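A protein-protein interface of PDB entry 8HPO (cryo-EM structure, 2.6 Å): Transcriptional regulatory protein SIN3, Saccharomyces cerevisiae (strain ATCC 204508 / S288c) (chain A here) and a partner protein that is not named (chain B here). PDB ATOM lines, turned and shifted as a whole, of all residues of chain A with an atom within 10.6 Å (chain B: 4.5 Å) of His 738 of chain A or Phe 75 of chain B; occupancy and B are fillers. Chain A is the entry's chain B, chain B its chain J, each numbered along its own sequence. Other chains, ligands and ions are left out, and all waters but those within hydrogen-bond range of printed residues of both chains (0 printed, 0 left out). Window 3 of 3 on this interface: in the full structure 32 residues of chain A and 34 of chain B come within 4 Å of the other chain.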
ATOM      1  N   GLU A 734      -7.720 -26.700  -5.211  1.00  0.00           N
ATOM      2  CA  GLU A 734      -6.505 -26.001  -5.603  1.00  0.00           C
ATOM      3  C   GLU A 734      -6.439 -24.677  -4.863  1.00  0.00           C
ATOM      4  O   GLU A 734      -7.342 -23.843  -4.988  1.00  0.00           O
ATOM      5  CB  GLU A 734      -6.451 -25.767  -7.113  1.00  0.00           C
ATOM      6  CG  GLU A 734      -7.779 -25.402  -7.735  1.00  0.00           C
ATOM      7  CD  GLU A 734      -7.768 -24.020  -8.336  1.00  0.00           C
ATOM      8  OE1 GLU A 734      -8.154 -23.878  -9.514  1.00  0.00           O
ATOM      9  OE2 GLU A 734      -7.363 -23.073  -7.635  1.00  0.00           O
ATOM     10  N   ASN A 735      -5.375 -24.488  -4.094  1.00  0.00           N
ATOM     11  CA  ASN A 735      -5.118 -23.233  -3.410  1.00  0.00           C
ATOM     12  C   ASN A 735      -4.099 -22.452  -4.221  1.00  0.00           C
ATOM     13  O   ASN A 735      -2.981 -22.928  -4.438  1.00  0.00           O
ATOM     14  CB  ASN A 735      -4.604 -23.467  -1.987  1.00  0.00           C
ATOM     15  CG  ASN A 735      -4.526 -22.185  -1.172  1.00  0.00           C
ATOM     16  OD1 ASN A 735      -3.850 -22.130  -0.145  1.00  0.00           O
ATOM     17  ND2 ASN A 735      -5.225 -21.150  -1.627  1.00  0.00           N
ATOM     18  N   ILE A 736      -4.489 -21.263  -4.680  1.00  0.00           N
ATOM     19  CA  ILE A 736      -3.518 -20.403  -5.335  1.00  0.00           C
ATOM     20  C   ILE A 736      -2.522 -19.938  -4.285  1.00  0.00           C
ATOM     21  O   ILE A 736      -2.839 -19.134  -3.400  1.00  0.00           O
ATOM     22  CB  ILE A 736      -4.211 -19.231  -6.050  1.00  0.00           C
ATOM     23  CG1 ILE A 736      -5.169 -18.502  -5.113  1.00  0.00           C
ATOM     24  CG2 ILE A 736      -4.957 -19.727  -7.276  1.00  0.00           C
ATOM     25  CD1 ILE A 736      -5.824 -17.313  -5.733  1.00  0.00           C
ATOM     26  N   VAL A 737      -1.313 -20.483  -4.354  1.00  0.00           N
ATOM     27  CA  VAL A 737      -0.323 -20.328  -3.301  1.00  0.00           C
ATOM     28  C   VAL A 737       0.462 -19.056  -3.575  1.00  0.00           C
ATOM     29  O   VAL A 737       0.425 -18.521  -4.688  1.00  0.00           O
ATOM     30  CB  VAL A 737       0.595 -21.561  -3.209  1.00  0.00           C
ATOM     31  CG1 VAL A 737       1.633 -21.555  -4.313  1.00  0.00           C
ATOM     32  CG2 VAL A 737       1.242 -21.651  -1.834  1.00  0.00           C
ATOM     33  N   HIS A 738       1.148 -18.561  -2.552  1.00  0.00           N
ATOM     34  CA  HIS A 738       1.852 -17.294  -2.654  1.00  0.00           C
ATOM     35  C   HIS A 738       3.209 -17.490  -3.319  1.00  0.00           C
ATOM     36  O   HIS A 738       3.696 -18.614  -3.455  1.00  0.00           O
ATOM     37  CB  HIS A 738       2.005 -16.703  -1.255  1.00  0.00           C
ATOM     38  CG  HIS A 738       2.558 -15.315  -1.230  1.00  0.00           C
ATOM     39  ND1 HIS A 738       3.909 -15.051  -1.267  1.00  0.00           N
ATOM     40  CD2 HIS A 738       1.941 -14.115  -1.150  1.00  0.00           C
ATOM     41  CE1 HIS A 738       4.100 -13.747  -1.220  1.00  0.00           C
ATOM     42  NE2 HIS A 738       2.922 -13.156  -1.146  1.00  0.00           N
ATOM     43  N   GLU A 739       3.813 -16.386  -3.751  1.00  0.00           N
ATOM     44  CA  GLU A 739       5.152 -16.444  -4.319  1.00  0.00           C
ATOM     45  C   GLU A 739       6.192 -16.425  -3.206  1.00  0.00           C
ATOM     46  O   GLU A 739       5.944 -15.904  -2.116  1.00  0.00           O
ATOM     47  CB  GLU A 739       5.363 -15.275  -5.281  1.00  0.00           C
ATOM     48  CG  GLU A 739       6.790 -15.074  -5.748  1.00  0.00           C
ATOM     49  CD  GLU A 739       7.096 -15.824  -7.017  1.00  0.00           C
ATOM     50  OE1 GLU A 739       6.498 -16.896  -7.233  1.00  0.00           O
ATOM     51  OE2 GLU A 739       7.951 -15.347  -7.785  1.00  0.00           O
ATOM     52  N   LYS A 740       7.359 -17.006  -3.481  1.00  0.00           N
ATOM     53  CA  LYS A 740       8.360 -17.186  -2.436  1.00  0.00           C
ATOM     54  C   LYS A 740       9.203 -15.932  -2.233  1.00  0.00           C
ATOM     55  O   LYS A 740       9.762 -15.722  -1.150  1.00  0.00           O
ATOM     56  CB  LYS A 740       9.258 -18.372  -2.783  1.00  0.00           C
ATOM     57  CG  LYS A 740       8.510 -19.671  -3.018  1.00  0.00           C
ATOM     58  CD  LYS A 740       9.455 -20.788  -3.431  1.00  0.00           C
ATOM     59  CE  LYS A 740      10.387 -20.353  -4.551  1.00  0.00           C
ATOM     60  NZ  LYS A 740       9.649 -19.799  -5.718  1.00  0.00           N
ATOM     61  N   HIS A 741       9.312 -15.088  -3.258  1.00  0.00           N
ATOM     62  CA  HIS A 741      10.456 -14.188  -3.327  1.00  0.00           C
ATOM     63  C   HIS A 741      10.194 -12.712  -3.051  1.00  0.00           C
ATOM     64  O   HIS A 741      10.798 -12.143  -2.138  1.00  0.00           O
ATOM     65  CB  HIS A 741      11.101 -14.302  -4.706  1.00  0.00           C
ATOM     66  CG  HIS A 741      11.617 -15.669  -5.020  1.00  0.00           C
ATOM     67  ND1 HIS A 741      12.887 -16.080  -4.679  1.00  0.00           N
ATOM     68  CD2 HIS A 741      11.036 -16.719  -5.645  1.00  0.00           C
ATOM     69  CE1 HIS A 741      13.066 -17.326  -5.081  1.00  0.00           C
ATOM     70  NE2 HIS A 741      11.958 -17.736  -5.671  1.00  0.00           N
ATOM     71  N   ARG A 742       9.271 -12.105  -3.797  1.00  0.00           N
ATOM     72  CA  ARG A 742       9.442 -10.750  -4.362  1.00  0.00           C
ATOM     73  C   ARG A 742      10.114  -9.805  -3.356  1.00  0.00           C
ATOM     74  O   ARG A 742      11.213  -9.312  -3.644  1.00  0.00           O
ATOM     75  CB  ARG A 742       8.096 -10.285  -4.934  1.00  0.00           C
ATOM     76  CG  ARG A 742       7.046  -9.743  -3.965  1.00  0.00           C
ATOM     77  CD  ARG A 742       6.341 -10.832  -3.169  1.00  0.00           C
ATOM     78  NE  ARG A 742       5.890 -10.328  -1.879  1.00  0.00           N
ATOM     79  CZ  ARG A 742       6.512 -10.570  -0.734  1.00  0.00           C
ATOM     80  NH1 ARG A 742       7.596 -11.330  -0.726  1.00  0.00           N
ATOM     81  NH2 ARG A 742       6.047 -10.067   0.400  1.00  0.00           N
ATOM     82  N   LEU A 743       9.517  -9.509  -2.202  1.00  0.00           N
ATOM     83  CA  LEU A 743      10.169  -8.646  -1.221  1.00  0.00           C
ATOM     84  C   LEU A 743       9.877  -9.012   0.229  1.00  0.00           C
ATOM     85  O   LEU A 743       9.564  -8.115   1.019  1.00  0.00           O
ATOM     86  CB  LEU A 743       9.801  -7.180  -1.474  1.00  0.00           C
ATOM     87  CG  LEU A 743      10.930  -6.205  -1.120  1.00  0.00           C
ATOM     88  CD1 LEU A 743      12.194  -6.550  -1.890  1.00  0.00           C
ATOM     89  CD2 LEU A 743      10.510  -4.780  -1.408  1.00  0.00           C
ATOM     90  N   ASP A 744       9.954 -10.288   0.596  1.00  0.00           N
ATOM     91  CA  ASP A 744       9.511 -10.806   1.904  1.00  0.00           C
ATOM     92  C   ASP A 744      10.084  -9.955   3.039  1.00  0.00           C
ATOM     93  O   ASP A 744       9.438  -9.848   4.093  1.00  0.00           O
ATOM     94  CB  ASP A 744       9.856 -12.289   1.966  1.00  0.00           C
ATOM     95  CG  ASP A 744      11.247 -12.584   1.443  1.00  0.00           C
ATOM     96  OD1 ASP A 744      11.364 -13.096   0.312  1.00  0.00           O
ATOM     97  OD2 ASP A 744      12.227 -12.298   2.163  1.00  0.00           O
ATOM     98  N   LEU A 745      11.253  -9.335   2.883  1.00  0.00           N
ATOM     99  CA  LEU A 745      12.049  -8.917   4.031  1.00  0.00           C
ATOM    100  C   LEU A 745      12.445  -7.443   4.032  1.00  0.00           C
ATOM    101  O   LEU A 745      12.693  -6.888   5.108  1.00  0.00           O
ATOM    102  CB  LEU A 745      13.322  -9.770   4.113  1.00  0.00           C
ATOM    103  CG  LEU A 745      14.495  -9.486   3.157  1.00  0.00           C
ATOM    104  CD1 LEU A 745      15.617 -10.498   3.370  1.00  0.00           C
ATOM    105  CD2 LEU A 745      14.094  -9.438   1.679  1.00  0.00           C
ATOM    106  N   SER B  71      -5.028 -18.339   2.064  1.00  0.00           N
ATOM    107  CA  SER B  71      -3.587 -18.348   2.303  1.00  0.00           C
ATOM    108  C   SER B  71      -2.958 -17.024   1.888  1.00  0.00           C
ATOM    109  O   SER B  71      -2.269 -16.376   2.683  1.00  0.00           O
ATOM    110  CB  SER B  71      -2.937 -19.510   1.554  1.00  0.00           C
ATOM    111  OG  SER B  71      -1.643 -19.158   1.099  1.00  0.00           O
ATOM    112  N   VAL B  72      -3.177 -16.616   0.635  1.00  0.00           N
ATOM    113  CA  VAL B  72      -2.632 -15.352   0.146  1.00  0.00           C
ATOM    114  C   VAL B  72      -3.113 -14.186   0.998  1.00  0.00           C
ATOM    115  O   VAL B  72      -2.362 -13.240   1.264  1.00  0.00           O
ATOM    116  CB  VAL B  72      -2.998 -15.154  -1.336  1.00  0.00           C
ATOM    117  CG1 VAL B  72      -2.376 -13.883  -1.872  1.00  0.00           C
ATOM    118  CG2 VAL B  72      -2.541 -16.340  -2.145  1.00  0.00           C
ATOM    119  N   LEU B  73      -4.364 -14.239   1.459  1.00  0.00           N
ATOM    120  CA  LEU B  73      -4.915 -13.090   2.167  1.00  0.00           C
ATOM    121  C   LEU B  73      -4.400 -13.034   3.601  1.00  0.00           C
ATOM    122  O   LEU B  73      -4.088 -11.951   4.113  1.00  0.00           O
ATOM    123  CB  LEU B  73      -6.442 -13.135   2.121  1.00  0.00           C
ATOM    124  CG  LEU B  73      -7.194 -11.801   2.133  1.00  0.00           C
ATOM    125  CD1 LEU B  73      -8.659 -12.045   1.822  1.00  0.00           C
ATOM    126  CD2 LEU B  73      -7.050 -11.053   3.452  1.00  0.00           C
ATOM    127  N   ALA B  74      -4.285 -14.189   4.260  1.00  0.00           N
ATOM    128  CA  ALA B  74      -3.583 -14.231   5.536  1.00  0.00           C
ATOM    129  C   ALA B  74      -2.155 -13.731   5.381  1.00  0.00           C
ATOM    130  O   ALA B  74      -1.644 -13.009   6.242  1.00  0.00           O
ATOM    131  CB  ALA B  74      -3.597 -15.649   6.100  1.00  0.00           C
ATOM    132  N   PHE B  75      -1.502 -14.092   4.274  1.00  0.00           N
ATOM    133  CA  PHE B  75      -0.139 -13.639   4.015  1.00  0.00           C
ATOM    134  C   PHE B  75      -0.070 -12.120   3.937  1.00  0.00           C
ATOM    135  O   PHE B  75       0.785 -11.491   4.572  1.00  0.00           O
ATOM    136  CB  PHE B  75       0.366 -14.278   2.719  1.00  0.00           C
ATOM    137  CG  PHE B  75       1.855 -14.213   2.530  1.00  0.00           C
ATOM    138  CD1 PHE B  75       2.501 -13.001   2.356  1.00  0.00           C
ATOM    139  CD2 PHE B  75       2.606 -15.373   2.500  1.00  0.00           C
ATOM    140  CE1 PHE B  75       3.862 -12.948   2.173  1.00  0.00           C
ATOM    141  CE2 PHE B  75       3.970 -15.326   2.316  1.00  0.00           C
ATOM    142  CZ  PHE B  75       4.598 -14.111   2.154  1.00  0.00           C
ATOM    143  N   THR B  76      -0.956 -11.510   3.149  1.00  0.00           N
ATOM    144  CA  THR B  76      -0.861 -10.066   2.966  1.00  0.00           C
ATOM    145  C   THR B  76      -1.351  -9.301   4.185  1.00  0.00           C
ATOM    146  O   THR B  76      -0.959  -8.145   4.370  1.00  0.00           O
ATOM    147  CB  THR B  76      -1.630  -9.607   1.725  1.00  0.00           C
ATOM    148  OG1 THR B  76      -1.704  -8.177   1.719  1.00  0.00           O
ATOM    149  CG2 THR B  76      -3.029 -10.160   1.728  1.00  0.00           C
ATOM    150  N   GLU B  77      -2.191  -9.910   5.024  1.00  0.00           N
ATOM    151  CA  GLU B  77      -2.511  -9.274   6.296  1.00  0.00           C
ATOM    152  C   GLU B  77      -1.360  -9.420   7.282  1.00  0.00           C
ATOM    153  O   GLU B  77      -1.153  -8.555   8.141  1.00  0.00           O
ATOM    154  CB  GLU B  77      -3.799  -9.859   6.871  1.00  0.00           C
ATOM    155  CG  GLU B  77      -5.073  -9.155   6.404  1.00  0.00           C
ATOM    156  CD  GLU B  77      -4.920  -7.647   6.275  1.00  0.00           C
ATOM    157  OE1 GLU B  77      -4.352  -7.011   7.190  1.00  0.00           O
ATOM    158  OE2 GLU B  77      -5.363  -7.092   5.248  1.00  0.00           O
ATOM    159  N   LYS B  78      -0.597 -10.507   7.165  1.00  0.00           N
ATOM    160  CA  LYS B  78       0.570 -10.714   8.014  1.00  0.00           C
ATOM    161  C   LYS B  78       1.670  -9.711   7.701  1.00  0.00           C
ATOM    162  O   LYS B  78       2.063  -8.909   8.555  1.00  0.00           O
ATOM    163  CB  LYS B  78       1.086 -12.141   7.830  1.00  0.00           C
ATOM    164  CG  LYS B  78       0.397 -13.185   8.681  1.00  0.00           C
ATOM    165  CD  LYS B  78       0.737 -12.996  10.142  1.00  0.00           C
ATOM    166  CE  LYS B  78       2.224 -13.209  10.361  1.00  0.00           C
ATOM    167  NZ  LYS B  78       2.719 -14.412   9.632  1.00  0.00           N
ATOM    168  N   HIS B  79       2.168  -9.731   6.468  1.00  0.00           N
ATOM    169  CA  HIS B  79       3.416  -9.052   6.151  1.00  0.00           C
ATOM    170  C   HIS B  79       3.225  -7.718   5.450  1.00  0.00           C
ATOM    171  O   HIS B  79       4.215  -7.018   5.206  1.00  0.00           O
ATOM    172  CB  HIS B  79       4.297  -9.967   5.303  1.00  0.00           C
ATOM    173  CG  HIS B  79       4.464 -11.333   5.889  1.00  0.00           C
ATOM    174  ND1 HIS B  79       5.293 -11.584   6.960  1.00  0.00           N
ATOM    175  CD2 HIS B  79       3.898 -12.518   5.564  1.00  0.00           C
ATOM    176  CE1 HIS B  79       5.236 -12.867   7.266  1.00  0.00           C
ATOM    177  NE2 HIS B  79       4.397 -13.456   6.434  1.00  0.00           N
ATOM    178  N   TYR B  80       1.991  -7.346   5.119  1.00  0.00           N
ATOM    179  CA  TYR B  80       1.665  -5.998   4.659  1.00  0.00           C
ATOM    180  C   TYR B  80       0.523  -5.446   5.504  1.00  0.00           C
ATOM    181  O   TYR B  80      -0.577  -5.194   4.994  1.00  0.00           O
ATOM    182  CB  TYR B  80       1.313  -5.980   3.174  1.00  0.00           C
ATOM    183  CG  TYR B  80       2.454  -6.415   2.295  1.00  0.00           C
ATOM    184  CD1 TYR B  80       3.544  -5.584   2.091  1.00  0.00           C
ATOM    185  CD2 TYR B  80       2.448  -7.654   1.676  1.00  0.00           C
ATOM    186  CE1 TYR B  80       4.596  -5.972   1.297  1.00  0.00           C
ATOM    187  CE2 TYR B  80       3.495  -8.052   0.878  1.00  0.00           C
ATOM    188  CZ  TYR B  80       4.569  -7.206   0.692  1.00  0.00           C
ATOM    189  OH  TYR B  80       5.621  -7.594  -0.105  1.00  0.00           O
ATOM    190  N   PRO B 234       0.191  -9.602  -3.640  1.00  0.00           N
ATOM    191  CA  PRO B 234       1.522 -10.024  -4.084  1.00  0.00           C
ATOM    192  C   PRO B 234       1.442 -11.054  -5.196  1.00  0.00           C
ATOM    193  O   PRO B 234       0.402 -11.670  -5.431  1.00  0.00           O
ATOM    194  CB  PRO B 234       2.147 -10.621  -2.819  1.00  0.00           C
ATOM    195  CG  PRO B 234       1.360 -10.065  -1.694  1.00  0.00           C
ATOM    196  CD  PRO B 234      -0.028  -9.913  -2.218  1.00  0.00           C
ATOM    197  N   THR B 235       2.566 -11.229  -5.888  1.00  0.00           N
ATOM    198  CA  THR B 235       2.665 -12.158  -7.005  1.00  0.00           C
ATOM    199  C   THR B 235       2.290 -13.566  -6.564  1.00  0.00           C
ATOM    200  O   THR B 235       2.558 -13.951  -5.424  1.00  0.00           O
ATOM    201  CB  THR B 235       4.081 -12.136  -7.586  1.00  0.00           C
ATOM    202  OG1 THR B 235       4.471 -10.783  -7.841  1.00  0.00           O
ATOM    203  CG2 THR B 235       4.147 -12.909  -8.883  1.00  0.00           C
ATOM    204  N   GLN B 237       2.555 -17.821  -7.234  1.00  0.00           N
ATOM    205  CA  GLN B 237       3.476 -18.770  -7.828  1.00  0.00           C
ATOM    206  C   GLN B 237       2.982 -19.128  -9.219  1.00  0.00           C
ATOM    207  O   GLN B 237       3.737 -19.049 -10.192  1.00  0.00           O
ATOM    208  CB  GLN B 237       3.609 -20.014  -6.954  1.00  0.00           C
ATOM    209  CG  GLN B 237       4.642 -21.000  -7.446  1.00  0.00           C
ATOM    210  CD  GLN B 237       6.029 -20.687  -6.932  1.00  0.00           C
ATOM    211  OE1 GLN B 237       7.013 -21.277  -7.376  1.00  0.00           O
ATOM    212  NE2 GLN B 237       6.118 -19.751  -5.991  1.00  0.00           N
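The side-chain hydroxyl (OH) of Tyr 80 of chain B lies within hydrogen-bond range of the guanidinium group (NH2) of Arg 742 of chain A. N of Glu 739 of chain A sits close to O of Thr 235 of chain B (3.2 Å). The backbone NH (N) of Gln 237 of chain B is in hydrogen-bond range of the backbone carbonyl oxygen (O) of Val 737 of chain A (3.4 Å). NE2 of Gln 237 of chain B sits at hydrogen-bond distance from OE1 of Glu 739 of chain A, 3.1 Å away. The side-chain amino group (NZ) of Lys 740 of chain A lies within hydrogen-bond range of the side-chain amide oxygen (OE1) of Gln 237 of chain B (3.4 Å).
Among the printed residues, pairs that only touch across the chains: Ile 736 of chain A with Val 72 of chain B (3.1 Å), His 738 of chain A with Pro 234 of chain B (3.1 Å), Asn 735 of chain A with Ser 71 of chain B (3.3 Å), His 738 of chain A with Phe 75 of chain B (3.4 Å), His 738 of chain A with Gln 237 of chain B (3.7 Å) and Arg 742 of chain A with Pro 234 of chain B (3.9 Å).
The side-chain amino group of Lys 740 of chain A sits at hydrogen-bond distance from a ring nitrogen (NE2) of His 741 of chain A, at 3.1 Å.
Of the printed residues of chain B, Asn 735 of chain A touches Ser 71. Printed residues of chain B within 4 Å of Val 737 of chain A: Gln 237. His 738 of chain A touches just these residues of chain B: Phe 75 (3.4 Å), Pro 234 (3.1 Å) and Gln 237 (3.7 Å). Of the printed residues of chain B, Lys 740 of chain A touches Gln 237 (3.4 Å). His 741 of chain A touches none of the printed residues of chain B. Printed residues of chain A within 4 Å of Ser 71 of chain B: Asn 735. Leu 73 of chain B touches none of the printed residues of chain A. No residue of chain A comes within 4 Å of Thr 76 of chain B. No residue of chain A comes within 4 Å of Lys 78 of chain B. No residue of chain A comes within 4 Å of His 79 of chain B. Of the printed residues of chain A, Tyr 80 of chain B touches Arg 742. Of the printed residues of chain A, Gln 237 of chain B touches Val 737, His 738, Glu 739 and Lys 740. The nearest residue of chain A that does not touch Phe 75 of chain B is Arg 742 of chain A (4.03 Å).
Among the printed residues, 11 pairs touch across the chains. Among the printed residues, no Asp or Glu carboxylate lies within 4 Å of a Lys or Arg side-chain nitrogen of the other chain.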
